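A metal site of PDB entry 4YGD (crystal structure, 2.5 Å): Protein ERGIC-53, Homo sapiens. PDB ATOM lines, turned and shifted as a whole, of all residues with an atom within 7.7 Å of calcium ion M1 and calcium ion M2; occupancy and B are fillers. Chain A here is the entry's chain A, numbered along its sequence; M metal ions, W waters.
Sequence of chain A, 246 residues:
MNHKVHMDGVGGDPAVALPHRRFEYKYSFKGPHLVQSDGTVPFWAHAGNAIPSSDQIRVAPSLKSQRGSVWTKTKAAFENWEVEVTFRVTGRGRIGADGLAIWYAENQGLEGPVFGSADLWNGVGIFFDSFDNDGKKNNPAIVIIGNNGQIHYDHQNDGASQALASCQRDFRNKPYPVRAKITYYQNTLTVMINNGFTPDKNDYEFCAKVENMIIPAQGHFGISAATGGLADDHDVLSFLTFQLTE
The side-chain carboxylate (OD2) of Asp 132 sits at hydrogen-bond distance from the backbone NH (N) of Lys 136 (3.2 Å). The side-chain carboxylate of Asp 132 lies within hydrogen-bond range of the backbone NH of Lys 137 (2.7 Å). The backbone carbonyl oxygen (O) of Asp 129 sits at hydrogen-bond distance from the side-chain amide nitrogen (ND2) of Asn 139 (3.2 Å). O of Ala 141 sits at hydrogen-bond distance from N of Asp 129, at 2.8 Å. The side-chain amide nitrogen of Gln 168 lies close to the backbone carbonyl oxygen of Asn 138, 3.4 Å away. N of Asp 134 sits at hydrogen-bond distance from O of Gln 156, at 3.0 Å.
Of the 28 residues printed, 5 come within 4 Å of calcium ion M1.
Within 4 Å of calcium ion M2: Asp 129, Phe 131, Asn 133 and Asp 158.
Calcium ion M1 is bound by OD2 of Asp 158 (2.2 Å), OD1 of Asp 132 (2.3 Å), OD1 of Asn 138 (2.4 Å), OD1 of Asn 139 (2.4 Å) and OD1 of Asp 134 (2.6 Å).
Calcium ion M2 is bound by the side-chain amide oxygen (OD1) of Asn 133 (2.3 Å), the backbone carbonyl oxygen (O) of Phe 131 (2.3 Å), the side-chain carboxylate (OD1) of Asp 158 (2.3 Å), the side-chain carboxylate (OD1) of Asp 129 (2.3 Å), water W1 (2.4 Å) and the side-chain carboxylate (OD2) of Asp 129 (2.7 Å).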
ATOM      1  N   GLY A  96     -10.329  35.818  16.034  1.00  0.00           N
ATOM      2  CA  GLY A  96     -10.823  35.222  17.272  1.00  0.00           C
ATOM      3  C   GLY A  96     -11.219  33.756  17.106  1.00  0.00           C
ATOM      4  O   GLY A  96     -11.189  33.232  16.016  1.00  0.00           O
ATOM      5  N   ALA A  97     -11.585  33.104  18.196  1.00  0.00           N
ATOM      6  CA  ALA A  97     -12.011  31.713  18.119  1.00  0.00           C
ATOM      7  C   ALA A  97     -12.743  31.310  19.394  1.00  0.00           C
ATOM      8  O   ALA A  97     -12.587  31.989  20.397  1.00  0.00           O
ATOM      9  CB  ALA A  97     -10.801  30.795  17.915  1.00  0.00           C
ATOM     10  N   ASP A  98     -13.534  30.255  19.364  1.00  0.00           N
ATOM     11  CA  ASP A  98     -13.880  29.496  18.158  1.00  0.00           C
ATOM     12  C   ASP A  98     -15.195  29.913  17.558  1.00  0.00           C
ATOM     13  O   ASP A  98     -15.380  29.829  16.348  1.00  0.00           O
ATOM     14  CB  ASP A  98     -13.966  28.000  18.460  1.00  0.00           C
ATOM     15  CG  ASP A  98     -12.636  27.295  18.290  1.00  0.00           C
ATOM     16  OD1 ASP A  98     -12.148  26.781  19.292  1.00  0.00           O
ATOM     17  OD2 ASP A  98     -12.088  27.275  17.157  1.00  0.00           O
ATOM     18  N   GLY A  99     -16.119  30.319  18.431  1.00  0.00           N
ATOM     19  CA  GLY A  99     -17.393  30.767  18.000  1.00  0.00           C
ATOM     20  C   GLY A  99     -18.473  30.167  18.852  1.00  0.00           C
ATOM     21  O   GLY A  99     -18.211  29.548  19.876  1.00  0.00           O
ATOM     22  N   PHE A 115     -18.346  23.261  19.100  1.00  0.00           N
ATOM     23  CA  PHE A 115     -18.537  24.518  19.786  1.00  0.00           C
ATOM     24  C   PHE A 115     -19.038  24.310  21.223  1.00  0.00           C
ATOM     25  O   PHE A 115     -19.995  24.923  21.668  1.00  0.00           O
ATOM     26  CB  PHE A 115     -19.470  25.369  18.972  1.00  0.00           C
ATOM     27  CG  PHE A 115     -18.914  25.738  17.646  1.00  0.00           C
ATOM     28  CD1 PHE A 115     -18.088  26.814  17.530  1.00  0.00           C
ATOM     29  CD2 PHE A 115     -19.218  25.015  16.518  1.00  0.00           C
ATOM     30  CE1 PHE A 115     -17.585  27.176  16.294  1.00  0.00           C
ATOM     31  CE2 PHE A 115     -18.704  25.375  15.282  1.00  0.00           C
ATOM     32  CZ  PHE A 115     -17.888  26.453  15.166  1.00  0.00           C
ATOM     33  N   PHE A 128     -21.827  29.992  14.384  1.00  0.00           N
ATOM     34  CA  PHE A 128     -21.174  31.279  14.202  1.00  0.00           C
ATOM     35  C   PHE A 128     -19.691  31.042  14.439  1.00  0.00           C
ATOM     36  O   PHE A 128     -19.193  31.063  15.555  1.00  0.00           O
ATOM     37  CB  PHE A 128     -21.749  32.285  15.185  1.00  0.00           C
ATOM     38  CG  PHE A 128     -23.221  32.520  14.997  1.00  0.00           C
ATOM     39  CD1 PHE A 128     -23.659  33.663  14.345  1.00  0.00           C
ATOM     40  CD2 PHE A 128     -24.136  31.596  15.398  1.00  0.00           C
ATOM     41  CE1 PHE A 128     -25.017  33.861  14.148  1.00  0.00           C
ATOM     42  CE2 PHE A 128     -25.493  31.797  15.222  1.00  0.00           C
ATOM     43  CZ  PHE A 128     -25.935  32.923  14.596  1.00  0.00           C
ATOM     44  N   ASP A 129     -18.990  30.819  13.344  1.00  0.00           N
ATOM     45  CA  ASP A 129     -17.660  30.257  13.359  1.00  0.00           C
ATOM     46  C   ASP A 129     -16.670  31.377  13.089  1.00  0.00           C
ATOM     47  O   ASP A 129     -16.580  31.886  11.972  1.00  0.00           O
ATOM     48  CB  ASP A 129     -17.601  29.187  12.255  1.00  0.00           C
ATOM     49  CG  ASP A 129     -16.359  28.373  12.281  1.00  0.00           C
ATOM     50  OD1 ASP A 129     -15.314  28.846  12.761  1.00  0.00           O
ATOM     51  OD2 ASP A 129     -16.404  27.230  11.799  1.00  0.00           O
ATOM     52  N   SER A 130     -15.969  31.771  14.121  1.00  0.00           N
ATOM     53  CA  SER A 130     -15.001  32.874  14.055  1.00  0.00           C
ATOM     54  C   SER A 130     -13.684  32.453  13.361  1.00  0.00           C
ATOM     55  O   SER A 130     -13.014  33.286  12.777  1.00  0.00           O
ATOM     56  CB  SER A 130     -14.585  33.264  15.473  1.00  0.00           C
ATOM     57  OG  SER A 130     -15.641  33.886  16.131  1.00  0.00           O
ATOM     58  N   PHE A 131     -13.299  31.179  13.507  1.00  0.00           N
ATOM     59  CA  PHE A 131     -11.944  30.808  13.193  1.00  0.00           C
ATOM     60  C   PHE A 131     -11.873  29.943  11.940  1.00  0.00           C
ATOM     61  O   PHE A 131     -12.487  28.855  11.859  1.00  0.00           O
ATOM     62  CB  PHE A 131     -11.261  30.125  14.375  1.00  0.00           C
ATOM     63  CG  PHE A 131      -9.784  29.891  14.163  1.00  0.00           C
ATOM     64  CD1 PHE A 131      -8.879  30.942  14.259  1.00  0.00           C
ATOM     65  CD2 PHE A 131      -9.301  28.619  13.825  1.00  0.00           C
ATOM     66  CE1 PHE A 131      -7.510  30.730  14.040  1.00  0.00           C
ATOM     67  CE2 PHE A 131      -7.942  28.413  13.593  1.00  0.00           C
ATOM     68  CZ  PHE A 131      -7.045  29.472  13.697  1.00  0.00           C
ATOM     69  N   ASP A 132     -11.057  30.448  11.011  1.00  0.00           N
ATOM     70  CA  ASP A 132     -10.822  29.892   9.678  1.00  0.00           C
ATOM     71  C   ASP A 132      -9.896  28.672   9.723  1.00  0.00           C
ATOM     72  O   ASP A 132      -8.716  28.766   9.437  1.00  0.00           O
ATOM     73  CB  ASP A 132     -10.209  30.992   8.802  1.00  0.00           C
ATOM     74  CG  ASP A 132     -10.231  30.681   7.334  1.00  0.00           C
ATOM     75  OD1 ASP A 132     -11.024  29.796   6.871  1.00  0.00           O
ATOM     76  OD2 ASP A 132      -9.454  31.376   6.639  1.00  0.00           O
ATOM     77  N   ASN A 133     -10.470  27.518  10.056  1.00  0.00           N
ATOM     78  CA  ASN A 133      -9.694  26.308  10.299  1.00  0.00           C
ATOM     79  C   ASN A 133      -9.018  25.771   9.022  1.00  0.00           C
ATOM     80  O   ASN A 133      -7.885  25.322   9.084  1.00  0.00           O
ATOM     81  CB  ASN A 133     -10.605  25.233  10.906  1.00  0.00           C
ATOM     82  CG  ASN A 133     -10.837  25.447  12.397  1.00  0.00           C
ATOM     83  OD1 ASN A 133     -11.815  26.062  12.820  1.00  0.00           O
ATOM     84  ND2 ASN A 133      -9.926  24.938  13.196  1.00  0.00           N
ATOM     85  N   ASP A 134      -9.729  25.847   7.893  1.00  0.00           N
ATOM     86  CA  ASP A 134      -9.215  25.401   6.597  1.00  0.00           C
ATOM     87  C   ASP A 134      -8.544  26.519   5.797  1.00  0.00           C
ATOM     88  O   ASP A 134      -8.405  26.408   4.576  1.00  0.00           O
ATOM     89  CB  ASP A 134     -10.358  24.817   5.755  1.00  0.00           C
ATOM     90  CG  ASP A 134     -11.547  25.798   5.562  1.00  0.00           C
ATOM     91  OD1 ASP A 134     -11.439  26.987   5.973  1.00  0.00           O
ATOM     92  OD2 ASP A 134     -12.577  25.385   4.998  1.00  0.00           O
ATOM     93  N   GLY A 135      -8.176  27.622   6.453  1.00  0.00           N
ATOM     94  CA  GLY A 135      -7.430  28.699   5.791  1.00  0.00           C
ATOM     95  C   GLY A 135      -7.978  29.315   4.517  1.00  0.00           C
ATOM     96  O   GLY A 135      -7.214  29.924   3.774  1.00  0.00           O
ATOM     97  N   LYS A 136      -9.295  29.203   4.283  1.00  0.00           N
ATOM     98  CA  LYS A 136      -9.951  29.757   3.075  1.00  0.00           C
ATOM     99  C   LYS A 136     -10.365  31.262   3.119  1.00  0.00           C
ATOM    100  O   LYS A 136     -11.128  31.704   2.250  1.00  0.00           O
ATOM    101  CB  LYS A 136     -11.196  28.921   2.708  1.00  0.00           C
ATOM    102  CG  LYS A 136     -10.941  27.456   2.394  1.00  0.00           C
ATOM    103  CD  LYS A 136     -10.198  27.247   1.081  1.00  0.00           C
ATOM    104  CE  LYS A 136      -9.732  25.793   0.902  1.00  0.00           C
ATOM    105  NZ  LYS A 136      -8.548  25.661   0.004  1.00  0.00           N
ATOM    106  N   LYS A 137      -9.857  32.020   4.093  1.00  0.00           N
ATOM    107  CA  LYS A 137     -10.119  33.467   4.247  1.00  0.00           C
ATOM    108  C   LYS A 137     -11.583  33.846   4.066  1.00  0.00           C
ATOM    109  O   LYS A 137     -11.914  34.880   3.508  1.00  0.00           O
ATOM    110  CB  LYS A 137      -9.193  34.303   3.333  1.00  0.00           C
ATOM    111  CG  LYS A 137      -7.740  33.885   3.444  1.00  0.00           C
ATOM    112  CD  LYS A 137      -6.727  34.936   3.107  1.00  0.00           C
ATOM    113  CE  LYS A 137      -5.421  34.167   3.212  1.00  0.00           C
ATOM    114  NZ  LYS A 137      -4.218  34.959   2.921  1.00  0.00           N
ATOM    115  N   ASN A 138     -12.458  32.990   4.585  1.00  0.00           N
ATOM    116  CA  ASN A 138     -13.903  33.202   4.495  1.00  0.00           C
ATOM    117  C   ASN A 138     -14.593  33.140   5.891  1.00  0.00           C
ATOM    118  O   ASN A 138     -15.635  32.493   6.058  1.00  0.00           O
ATOM    119  CB  ASN A 138     -14.478  32.155   3.542  1.00  0.00           C
ATOM    120  CG  ASN A 138     -14.143  30.755   3.976  1.00  0.00           C
ATOM    121  OD1 ASN A 138     -13.245  30.547   4.811  1.00  0.00           O
ATOM    122  ND2 ASN A 138     -14.896  29.789   3.488  1.00  0.00           N
ATOM    123  N   ASN A 139     -13.987  33.801   6.889  1.00  0.00           N
ATOM    124  CA  ASN A 139     -14.512  33.854   8.256  1.00  0.00           C
ATOM    125  C   ASN A 139     -14.381  35.278   8.781  1.00  0.00           C
ATOM    126  O   ASN A 139     -13.502  35.992   8.363  1.00  0.00           O
ATOM    127  CB  ASN A 139     -13.757  32.912   9.209  1.00  0.00           C
ATOM    128  CG  ASN A 139     -13.918  31.443   8.834  1.00  0.00           C
ATOM    129  OD1 ASN A 139     -13.292  30.974   7.881  1.00  0.00           O
ATOM    130  ND2 ASN A 139     -14.718  30.698   9.607  1.00  0.00           N
ATOM    131  N   PRO A 140     -15.224  35.673   9.733  1.00  0.00           N
ATOM    132  CA  PRO A 140     -16.266  34.881  10.364  1.00  0.00           C
ATOM    133  C   PRO A 140     -17.385  34.469   9.419  1.00  0.00           C
ATOM    134  O   PRO A 140     -17.695  35.177   8.478  1.00  0.00           O
ATOM    135  CB  PRO A 140     -16.787  35.814  11.438  1.00  0.00           C
ATOM    136  CG  PRO A 140     -15.604  36.652  11.803  1.00  0.00           C
ATOM    137  CD  PRO A 140     -14.950  36.921  10.479  1.00  0.00           C
ATOM    138  N   ALA A 141     -17.945  33.295   9.663  1.00  0.00           N
ATOM    139  CA  ALA A 141     -19.022  32.759   8.873  1.00  0.00           C
ATOM    140  C   ALA A 141     -20.115  32.225   9.755  1.00  0.00           C
ATOM    141  O   ALA A 141     -19.900  31.883  10.890  1.00  0.00           O
ATOM    142  CB  ALA A 141     -18.510  31.629   7.942  1.00  0.00           C
ATOM    143  N   TYR A 153     -19.088  16.241  12.979  1.00  0.00           N
ATOM    144  CA  TYR A 153     -18.794  17.593  12.525  1.00  0.00           C
ATOM    145  C   TYR A 153     -17.324  17.767  12.072  1.00  0.00           C
ATOM    146  O   TYR A 153     -16.371  17.459  12.793  1.00  0.00           O
ATOM    147  CB  TYR A 153     -19.167  18.650  13.592  1.00  0.00           C
ATOM    148  CG  TYR A 153     -18.631  20.050  13.265  1.00  0.00           C
ATOM    149  CD1 TYR A 153     -19.182  20.827  12.250  1.00  0.00           C
ATOM    150  CD2 TYR A 153     -17.567  20.579  13.976  1.00  0.00           C
ATOM    151  CE1 TYR A 153     -18.672  22.087  11.967  1.00  0.00           C
ATOM    152  CE2 TYR A 153     -17.039  21.826  13.699  1.00  0.00           C
ATOM    153  CZ  TYR A 153     -17.578  22.575  12.701  1.00  0.00           C
ATOM    154  OH  TYR A 153     -17.051  23.820  12.438  1.00  0.00           O
ATOM    155  N   ASP A 154     -17.178  18.338  10.886  1.00  0.00           N
ATOM    156  CA  ASP A 154     -15.896  18.559  10.263  1.00  0.00           C
ATOM    157  C   ASP A 154     -15.272  19.893  10.701  1.00  0.00           C
ATOM    158  O   ASP A 154     -15.353  20.904   9.996  1.00  0.00           O
ATOM    159  CB  ASP A 154     -16.087  18.511   8.729  1.00  0.00           C
ATOM    160  CG  ASP A 154     -14.774  18.389   7.972  1.00  0.00           C
ATOM    161  OD1 ASP A 154     -13.720  18.193   8.605  1.00  0.00           O
ATOM    162  OD2 ASP A 154     -14.797  18.562   6.731  1.00  0.00           O
ATOM    163  N   HIS A 155     -14.677  19.884  11.894  1.00  0.00           N
ATOM    164  CA  HIS A 155     -13.949  21.022  12.463  1.00  0.00           C
ATOM    165  C   HIS A 155     -12.939  21.674  11.539  1.00  0.00           C
ATOM    166  O   HIS A 155     -12.872  22.893  11.440  1.00  0.00           O
ATOM    167  CB  HIS A 155     -13.119  20.542  13.657  1.00  0.00           C
ATOM    168  CG  HIS A 155     -13.937  19.978  14.778  1.00  0.00           C
ATOM    169  ND1 HIS A 155     -14.538  20.773  15.729  1.00  0.00           N
ATOM    170  CD2 HIS A 155     -14.225  18.695  15.106  1.00  0.00           C
ATOM    171  CE1 HIS A 155     -15.168  19.997  16.602  1.00  0.00           C
ATOM    172  NE2 HIS A 155     -14.994  18.738  16.244  1.00  0.00           N
ATOM    173  N   GLN A 156     -12.111  20.858  10.905  1.00  0.00           N
ATOM    174  CA  GLN A 156     -10.980  21.373  10.128  1.00  0.00           C
ATOM    175  C   GLN A 156     -11.400  22.187   8.935  1.00  0.00           C
ATOM    176  O   GLN A 156     -10.687  23.092   8.527  1.00  0.00           O
ATOM    177  CB  GLN A 156     -10.073  20.224   9.690  1.00  0.00           C
ATOM    178  CG  GLN A 156      -9.369  19.577  10.892  1.00  0.00           C
ATOM    179  CD  GLN A 156      -9.974  18.228  11.296  1.00  0.00           C
ATOM    180  OE1 GLN A 156     -11.176  17.966  11.121  1.00  0.00           O
ATOM    181  NE2 GLN A 156      -9.130  17.366  11.863  1.00  0.00           N
ATOM    182  N   ASN A 157     -12.562  21.861   8.374  1.00  0.00           N
ATOM    183  CA  ASN A 157     -13.082  22.573   7.199  1.00  0.00           C
ATOM    184  C   ASN A 157     -14.223  23.516   7.509  1.00  0.00           C
ATOM    185  O   ASN A 157     -14.977  23.919   6.591  1.00  0.00           O
ATOM    186  CB  ASN A 157     -13.490  21.575   6.115  1.00  0.00           C
ATOM    187  CG  ASN A 157     -12.314  20.735   5.650  1.00  0.00           C
ATOM    188  OD1 ASN A 157     -11.464  21.206   4.888  1.00  0.00           O
ATOM    189  ND2 ASN A 157     -12.236  19.495   6.122  1.00  0.00           N
ATOM    190  N   ASP A 158     -14.383  23.891   8.782  1.00  0.00           N
ATOM    191  CA  ASP A 158     -15.467  24.808   9.160  1.00  0.00           C
ATOM    192  C   ASP A 158     -16.824  24.292   8.688  1.00  0.00           C
ATOM    193  O   ASP A 158     -17.669  25.064   8.236  1.00  0.00           O
ATOM    194  CB  ASP A 158     -15.212  26.212   8.578  1.00  0.00           C
ATOM    195  CG  ASP A 158     -13.952  26.829   9.098  1.00  0.00           C
ATOM    196  OD1 ASP A 158     -13.593  26.483  10.243  1.00  0.00           O
ATOM    197  OD2 ASP A 158     -13.340  27.680   8.401  1.00  0.00           O
ATOM    198  N   GLY A 159     -17.000  22.979   8.728  1.00  0.00           N
ATOM    199  CA  GLY A 159     -18.181  22.312   8.152  1.00  0.00           C
ATOM    200  C   GLY A 159     -18.524  22.582   6.696  1.00  0.00           C
ATOM    201  O   GLY A 159     -19.671  22.341   6.283  1.00  0.00           O
ATOM    202  N   ALA A 160     -17.566  23.030   5.891  1.00  0.00           N
ATOM    203  CA  ALA A 160     -17.841  23.472   4.498  1.00  0.00           C
ATOM    204  C   ALA A 160     -18.552  22.451   3.617  1.00  0.00           C
ATOM    205  O   ALA A 160     -19.407  22.821   2.807  1.00  0.00           O
ATOM    206  CB  ALA A 160     -16.564  23.944   3.797  1.00  0.00           C
ATOM    207  N   GLN A 168     -21.276  34.876   4.909  1.00  0.00           N
ATOM    208  CA  GLN A 168     -20.129  35.489   5.555  1.00  0.00           C
ATOM    209  C   GLN A 168     -20.613  36.736   6.246  1.00  0.00           C
ATOM    210  O   GLN A 168     -21.366  37.469   5.691  1.00  0.00           O
ATOM    211  CB  GLN A 168     -19.066  35.800   4.540  1.00  0.00           C
ATOM    212  CG  GLN A 168     -18.442  34.528   3.998  1.00  0.00           C
ATOM    213  CD  GLN A 168     -17.046  34.779   3.568  1.00  0.00           C
ATOM    214  OE1 GLN A 168     -16.653  34.450   2.451  1.00  0.00           O
ATOM    215  NE2 GLN A 168     -16.268  35.428   4.439  1.00  0.00           N
HETATM  216 CA    CA M   1     -13.131  28.907   6.583  1.00  0.00          CA
HETATM  217 CA    CA M   2     -13.815  27.076  12.483  1.00  0.00          CA
HETATM  218  O   HOH W   1     -13.582  27.584  14.814  1.00  0.00           O
